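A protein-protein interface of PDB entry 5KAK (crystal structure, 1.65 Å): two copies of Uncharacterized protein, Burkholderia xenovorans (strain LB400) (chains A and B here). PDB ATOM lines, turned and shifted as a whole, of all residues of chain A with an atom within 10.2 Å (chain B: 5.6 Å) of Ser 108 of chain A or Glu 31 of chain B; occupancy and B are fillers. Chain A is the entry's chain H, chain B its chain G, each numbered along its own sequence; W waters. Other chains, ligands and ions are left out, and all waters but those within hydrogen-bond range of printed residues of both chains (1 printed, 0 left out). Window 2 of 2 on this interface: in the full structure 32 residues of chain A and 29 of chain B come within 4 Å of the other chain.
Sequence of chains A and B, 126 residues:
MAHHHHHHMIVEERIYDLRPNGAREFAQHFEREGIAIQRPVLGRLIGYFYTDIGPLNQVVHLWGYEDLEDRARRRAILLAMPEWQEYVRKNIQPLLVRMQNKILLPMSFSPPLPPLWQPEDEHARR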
ATOM      1  N   HIS A   6      12.511   9.023  20.251  1.00  0.00           N
ATOM      2  CA  HIS A   6      13.889   8.580  20.449  1.00  0.00           C
ATOM      3  C   HIS A   6      14.455   9.052  21.789  1.00  0.00           C
ATOM      4  O   HIS A   6      15.632   8.829  22.075  1.00  0.00           O
ATOM      5  CB  HIS A   6      14.788   9.070  19.306  1.00  0.00           C
ATOM      6  CG  HIS A   6      14.766   8.189  18.095  1.00  0.00           C
ATOM      7  ND1 HIS A   6      15.639   7.135  17.926  1.00  0.00           N
ATOM      8  CD2 HIS A   6      13.981   8.209  16.991  1.00  0.00           C
ATOM      9  CE1 HIS A   6      15.391   6.543  16.771  1.00  0.00           C
ATOM     10  NE2 HIS A   6      14.386   7.172  16.187  1.00  0.00           N
ATOM     11  N   HIS A   7      13.604   9.699  22.594  1.00  0.00           N
ATOM     12  CA  HIS A   7      13.950  10.207  23.923  1.00  0.00           C
ATOM     13  C   HIS A   7      15.356  10.794  24.002  1.00  0.00           C
ATOM     14  O   HIS A   7      16.202  10.289  24.747  1.00  0.00           O
ATOM     15  CB  HIS A   7      13.798   9.103  24.972  1.00  0.00           C
ATOM     16  N   MET A   9      17.955  10.642  22.370  1.00  0.00           N
ATOM     17  CA  MET A   9      19.108   9.873  21.915  1.00  0.00           C
ATOM     18  C   MET A   9      19.937  10.700  20.939  1.00  0.00           C
ATOM     19  O   MET A   9      19.403  11.471  20.141  1.00  0.00           O
ATOM     20  CB  MET A   9      18.649   8.566  21.244  1.00  0.00           C
ATOM     21  CG  MET A   9      19.382   8.201  19.930  1.00  0.00           C
ATOM     22  SD  MET A   9      18.639   6.844  18.946  1.00  0.00           S
ATOM     23  CE  MET A   9      19.863   6.651  17.643  1.00  0.00           C
ATOM     24  N   LEU A 105      21.447  13.944  15.355  1.00  0.00           N
ATOM     25  CA  LEU A 105      20.188  13.628  16.019  1.00  0.00           C
ATOM     26  C   LEU A 105      19.323  12.803  15.086  1.00  0.00           C
ATOM     27  O   LEU A 105      19.175  13.169  13.914  1.00  0.00           O
ATOM     28  CB  LEU A 105      19.447  14.902  16.422  1.00  0.00           C
ATOM     29  CG  LEU A 105      20.265  15.866  17.282  1.00  0.00           C
ATOM     30  CD1 LEU A 105      19.384  17.031  17.663  1.00  0.00           C
ATOM     31  CD2 LEU A 105      20.807  15.163  18.513  1.00  0.00           C
ATOM     32  N   PRO A 106      18.755  11.693  15.549  1.00  0.00           N
ATOM     33  CA  PRO A 106      18.016  10.805  14.641  1.00  0.00           C
ATOM     34  C   PRO A 106      16.640  11.361  14.281  1.00  0.00           C
ATOM     35  O   PRO A 106      15.928  11.916  15.119  1.00  0.00           O
ATOM     36  CB  PRO A 106      17.898   9.505  15.445  1.00  0.00           C
ATOM     37  CG  PRO A 106      17.945   9.953  16.888  1.00  0.00           C
ATOM     38  CD  PRO A 106      18.925  11.117  16.895  1.00  0.00           C
ATOM     39  N   MET A 107      16.263  11.209  13.017  1.00  0.00           N
ATOM     40  CA  MET A 107      14.887  11.514  12.649  1.00  0.00           C
ATOM     41  C   MET A 107      13.953  10.423  13.170  1.00  0.00           C
ATOM     42  O   MET A 107      14.381   9.332  13.546  1.00  0.00           O
ATOM     43  CB  MET A 107      14.764  11.666  11.139  1.00  0.00           C
ATOM     44  CG  MET A 107      15.577  12.835  10.615  1.00  0.00           C
ATOM     45  SD  MET A 107      15.441  12.993   8.846  1.00  0.00           S
ATOM     46  CE  MET A 107      16.636  14.270   8.547  1.00  0.00           C
ATOM     47  N   SER A 108      12.650  10.731  13.189  1.00  0.00           N
ATOM     48  CA  SER A 108      11.703   9.874  13.904  1.00  0.00           C
ATOM     49  C   SER A 108      11.642   8.463  13.330  1.00  0.00           C
ATOM     50  O   SER A 108      11.362   7.512  14.065  1.00  0.00           O
ATOM     51  CB  SER A 108      10.313  10.497  13.877  1.00  0.00           C
ATOM     52  OG  SER A 108       9.909  10.691  12.542  1.00  0.00           O
ATOM     53  N   PHE A 109      11.879   8.303  12.033  1.00  0.00           N
ATOM     54  CA  PHE A 109      11.839   6.993  11.390  1.00  0.00           C
ATOM     55  C   PHE A 109      13.196   6.298  11.392  1.00  0.00           C
ATOM     56  O   PHE A 109      13.311   5.174  10.893  1.00  0.00           O
ATOM     57  CB  PHE A 109      11.339   7.133   9.947  1.00  0.00           C
ATOM     58  CG  PHE A 109      12.139   8.107   9.130  1.00  0.00           C
ATOM     59  CD1 PHE A 109      13.326   7.722   8.537  1.00  0.00           C
ATOM     60  CD2 PHE A 109      11.712   9.416   8.977  1.00  0.00           C
ATOM     61  CE1 PHE A 109      14.064   8.608   7.806  1.00  0.00           C
ATOM     62  CE2 PHE A 109      12.450  10.310   8.235  1.00  0.00           C
ATOM     63  CZ  PHE A 109      13.630   9.907   7.651  1.00  0.00           C
ATOM     64  N   SER A 110      14.218   6.937  11.930  1.00  0.00           N
ATOM     65  CA  SER A 110      15.528   6.317  11.995  1.00  0.00           C
ATOM     66  C   SER A 110      15.496   5.167  13.002  1.00  0.00           C
ATOM     67  O   SER A 110      14.693   5.178  13.933  1.00  0.00           O
ATOM     68  CB  SER A 110      16.570   7.360  12.395  1.00  0.00           C
ATOM     69  OG  SER A 110      17.894   6.898  12.165  1.00  0.00           O
ATOM     70  N   PRO A 111      16.329   4.147  12.819  1.00  0.00           N
ATOM     71  CA  PRO A 111      16.321   2.994  13.741  1.00  0.00           C
ATOM     72  C   PRO A 111      16.575   3.418  15.175  1.00  0.00           C
ATOM     73  O   PRO A 111      17.207   4.457  15.429  1.00  0.00           O
ATOM     74  CB  PRO A 111      17.476   2.128  13.215  1.00  0.00           C
ATOM     75  CG  PRO A 111      17.517   2.426  11.784  1.00  0.00           C
ATOM     76  CD  PRO A 111      17.214   3.904  11.668  1.00  0.00           C
ATOM     77  N   PRO A 112      16.112   2.635  16.145  1.00  0.00           N
ATOM     78  CA  PRO A 112      16.457   2.909  17.545  1.00  0.00           C
ATOM     79  C   PRO A 112      17.935   2.649  17.819  1.00  0.00           C
ATOM     80  O   PRO A 112      18.656   2.039  17.024  1.00  0.00           O
ATOM     81  CB  PRO A 112      15.564   1.940  18.335  1.00  0.00           C
ATOM     82  CG  PRO A 112      15.235   0.844  17.360  1.00  0.00           C
ATOM     83  CD  PRO A 112      15.182   1.503  16.000  1.00  0.00           C
ATOM     84  N   LEU A 113      18.371   3.121  18.990  1.00  0.00           N
ATOM     85  CA  LEU A 113      19.715   2.855  19.487  1.00  0.00           C
ATOM     86  C   LEU A 113      20.006   1.356  19.496  1.00  0.00           C
ATOM     87  O   LEU A 113      19.110   0.552  19.774  1.00  0.00           O
ATOM     88  CB  LEU A 113      19.877   3.400  20.910  1.00  0.00           C
ATOM     89  CG  LEU A 113      20.382   4.828  21.096  1.00  0.00           C
ATOM     90  CD1 LEU A 113      20.642   5.128  22.568  1.00  0.00           C
ATOM     91  CD2 LEU A 113      21.626   5.034  20.270  1.00  0.00           C
ATOM     92  N   PHE B  26      12.646  19.323   6.047  1.00  0.00           N
ATOM     93  CA  PHE B  26      13.167  18.150   5.361  1.00  0.00           C
ATOM     94  C   PHE B  26      12.735  16.872   6.058  1.00  0.00           C
ATOM     95  O   PHE B  26      12.267  15.925   5.413  1.00  0.00           O
ATOM     96  CB  PHE B  26      14.692  18.253   5.306  1.00  0.00           C
ATOM     97  CG  PHE B  26      15.372  17.180   4.501  1.00  0.00           C
ATOM     98  CD1 PHE B  26      15.586  15.917   5.034  1.00  0.00           C
ATOM     99  CD2 PHE B  26      15.873  17.459   3.235  1.00  0.00           C
ATOM    100  CE1 PHE B  26      16.228  14.937   4.302  1.00  0.00           C
ATOM    101  CE2 PHE B  26      16.535  16.495   2.504  1.00  0.00           C
ATOM    102  CZ  PHE B  26      16.724  15.237   3.035  1.00  0.00           C
ATOM    103  N   ALA B  27      12.919  16.819   7.380  1.00  0.00           N
ATOM    104  CA  ALA B  27      12.496  15.655   8.154  1.00  0.00           C
ATOM    105  C   ALA B  27      10.983  15.480   8.120  1.00  0.00           C
ATOM    106  O   ALA B  27      10.484  14.351   7.988  1.00  0.00           O
ATOM    107  CB  ALA B  27      12.994  15.777   9.594  1.00  0.00           C
ATOM    108  N   GLN B  28      10.233  16.579   8.239  1.00  0.00           N
ATOM    109  CA  GLN B  28       8.774  16.478   8.197  1.00  0.00           C
ATOM    110  C   GLN B  28       8.305  15.801   6.914  1.00  0.00           C
ATOM    111  O   GLN B  28       7.485  14.878   6.962  1.00  0.00           O
ATOM    112  CB  GLN B  28       8.141  17.858   8.343  1.00  0.00           C
ATOM    113  CG  GLN B  28       8.333  18.475   9.707  1.00  0.00           C
ATOM    114  CD  GLN B  28       7.788  19.890   9.778  1.00  0.00           C
ATOM    115  OE1 GLN B  28       7.687  20.580   8.761  1.00  0.00           O
ATOM    116  NE2 GLN B  28       7.430  20.330  10.981  1.00  0.00           N
ATOM    117  N   HIS B  29       8.826  16.231   5.755  1.00  0.00           N
ATOM    118  CA  HIS B  29       8.423  15.590   4.501  1.00  0.00           C
ATOM    119  C   HIS B  29       8.771  14.106   4.501  1.00  0.00           C
ATOM    120  O   HIS B  29       8.015  13.282   3.977  1.00  0.00           O
ATOM    121  CB  HIS B  29       9.086  16.257   3.288  1.00  0.00           C
ATOM    122  CG  HIS B  29       8.567  17.624   2.974  1.00  0.00           C
ATOM    123  ND1 HIS B  29       7.226  17.890   2.784  1.00  0.00           N
ATOM    124  CD2 HIS B  29       9.216  18.798   2.792  1.00  0.00           C
ATOM    125  CE1 HIS B  29       7.073  19.175   2.512  1.00  0.00           C
ATOM    126  NE2 HIS B  29       8.266  19.746   2.503  1.00  0.00           N
ATOM    127  N   PHE B  30       9.943  13.740   5.032  1.00  0.00           N
ATOM    128  CA  PHE B  30      10.313  12.333   4.937  1.00  0.00           C
ATOM    129  C   PHE B  30       9.484  11.467   5.873  1.00  0.00           C
ATOM    130  O   PHE B  30       9.161  10.329   5.524  1.00  0.00           O
ATOM    131  CB  PHE B  30      11.815  12.154   5.177  1.00  0.00           C
ATOM    132  CG  PHE B  30      12.611  12.199   3.908  1.00  0.00           C
ATOM    133  CD1 PHE B  30      12.721  11.064   3.105  1.00  0.00           C
ATOM    134  CD2 PHE B  30      13.196  13.382   3.476  1.00  0.00           C
ATOM    135  CE1 PHE B  30      13.417  11.099   1.925  1.00  0.00           C
ATOM    136  CE2 PHE B  30      13.899  13.427   2.284  1.00  0.00           C
ATOM    137  CZ  PHE B  30      14.008  12.285   1.503  1.00  0.00           C
ATOM    138  N   GLU B  31       9.109  11.973   7.045  1.00  0.00           N
ATOM    139  CA  GLU B  31       8.262  11.158   7.900  1.00  0.00           C
ATOM    140  C   GLU B  31       6.840  11.070   7.353  1.00  0.00           C
ATOM    141  O   GLU B  31       6.232   9.995   7.398  1.00  0.00           O
ATOM    142  CB  GLU B  31       8.282  11.686   9.333  1.00  0.00           C
ATOM    143  CG  GLU B  31       7.973  13.152   9.485  1.00  0.00           C
ATOM    144  CD  GLU B  31       8.121  13.610  10.914  1.00  0.00           C
ATOM    145  OE1 GLU B  31       8.692  12.846  11.722  1.00  0.00           O
ATOM    146  OE2 GLU B  31       7.660  14.727  11.233  1.00  0.00           O
ATOM    147  N   ARG B  32       6.302  12.172   6.824  1.00  0.00           N
ATOM    148  CA  ARG B  32       4.929  12.186   6.324  1.00  0.00           C
ATOM    149  C   ARG B  32       4.762  11.372   5.052  1.00  0.00           C
ATOM    150  O   ARG B  32       3.706  10.771   4.840  1.00  0.00           O
ATOM    151  CB  ARG B  32       4.473  13.618   6.053  1.00  0.00           C
ATOM    152  CG  ARG B  32       4.178  14.450   7.282  1.00  0.00           C
ATOM    153  CD  ARG B  32       3.329  15.671   6.910  1.00  0.00           C
ATOM    154  NE  ARG B  32       3.939  16.929   7.335  1.00  0.00           N
ATOM    155  CZ  ARG B  32       4.598  17.755   6.529  1.00  0.00           C
ATOM    156  NH1 ARG B  32       5.115  18.873   7.016  1.00  0.00           N
ATOM    157  NH2 ARG B  32       4.737  17.471   5.239  1.00  0.00           N
ATOM    158  N   GLU B  33       5.773  11.351   4.189  1.00  0.00           N
ATOM    159  CA  GLU B  33       5.559  10.890   2.829  1.00  0.00           C
ATOM    160  C   GLU B  33       6.813  10.262   2.228  1.00  0.00           C
ATOM    161  O   GLU B  33       6.739   9.240   1.538  1.00  0.00           O
ATOM    162  CB  GLU B  33       5.084  12.071   1.988  1.00  0.00           C
ATOM    163  CG  GLU B  33       4.679  11.726   0.585  1.00  0.00           C
ATOM    164  CD  GLU B  33       4.405  12.966  -0.236  1.00  0.00           C
ATOM    165  OE1 GLU B  33       4.438  14.076   0.344  1.00  0.00           O
ATOM    166  OE2 GLU B  33       4.172  12.830  -1.455  1.00  0.00           O
ATOM    167  N   GLY B  34       7.973  10.855   2.499  1.00  0.00           N
ATOM    168  CA  GLY B  34       9.159  10.506   1.737  1.00  0.00           C
ATOM    169  C   GLY B  34       9.733   9.142   2.062  1.00  0.00           C
ATOM    170  O   GLY B  34      10.118   8.394   1.156  1.00  0.00           O
ATOM    171  N   ILE B  35       9.848   8.810   3.350  1.00  0.00           N
ATOM    172  CA  ILE B  35      10.553   7.587   3.683  1.00  0.00           C
ATOM    173  C   ILE B  35       9.706   6.368   3.328  1.00  0.00           C
ATOM    174  O   ILE B  35      10.259   5.299   3.065  1.00  0.00           O
ATOM    175  CB  ILE B  35      11.004   7.572   5.158  1.00  0.00           C
ATOM    176  CG1 ILE B  35      12.129   6.553   5.342  1.00  0.00           C
ATOM    177  CG2 ILE B  35       9.847   7.327   6.110  1.00  0.00           C
ATOM    178  CD1 ILE B  35      13.388   6.952   4.609  1.00  0.00           C
HETATM  179  O   HOH W   1      12.025  13.300  12.259  1.00  0.00           O
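The side-chain carboxylate (OE1) of Glu 31 of chain B is in hydrogen-bond range of the side-chain hydroxyl (OG) of Ser 108 of chain A, 2.6 Å away.
N of Ile 35 of chain B sits at hydrogen-bond distance from O of Phe 30 of chain B (2.7 Å).
A ring nitrogen (NE2) of His 6 of chain A lies within hydrogen-bond range of the backbone carbonyl oxygen (O) of Met 107 of chain A (3.4 Å).
Among the printed residues, merely in contact across the chains: Phe 109 of chain A with Ile 35 of chain B (3.6 Å), Phe 109 of chain A with Phe 30 of chain B (3.6 Å), Met 107 of chain A with Ala 27 of chain B (3.8 Å) and Phe 109 of chain A with Glu 31 of chain B (3.9 Å).
Of the printed residues of chain B, Ser 108 of chain A touches Glu 31 (2.6 Å).
Printed residues of chain A within 4 Å of Glu 31 of chain B: Ser 108 and Phe 109.
Printed residues of chain A within 4 Å of Ile 35 of chain B: Phe 109 (3.6 Å).
Of the printed residues of chain B, Met 107 of chain A touches Ala 27 (3.8 Å).
Printed residues of chain B within 4 Å of Phe 109 of chain A: Phe 30 (3.6 Å), Glu 31 (3.9 Å) and Ile 35 (3.6 Å).
Of the 12 printed residues of chain A, 3 touch a printed residue of chain B.
Printed residues of chain A that touch a printed residue of chain B: Met 107, Ser 108 and Phe 109.
Among the printed residues, 5 pairs touch across the chains.
No position is printed for both chains.
Water W1 bridges N of Ser 108 of chain A and OE1 of Glu 31 of chain B.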
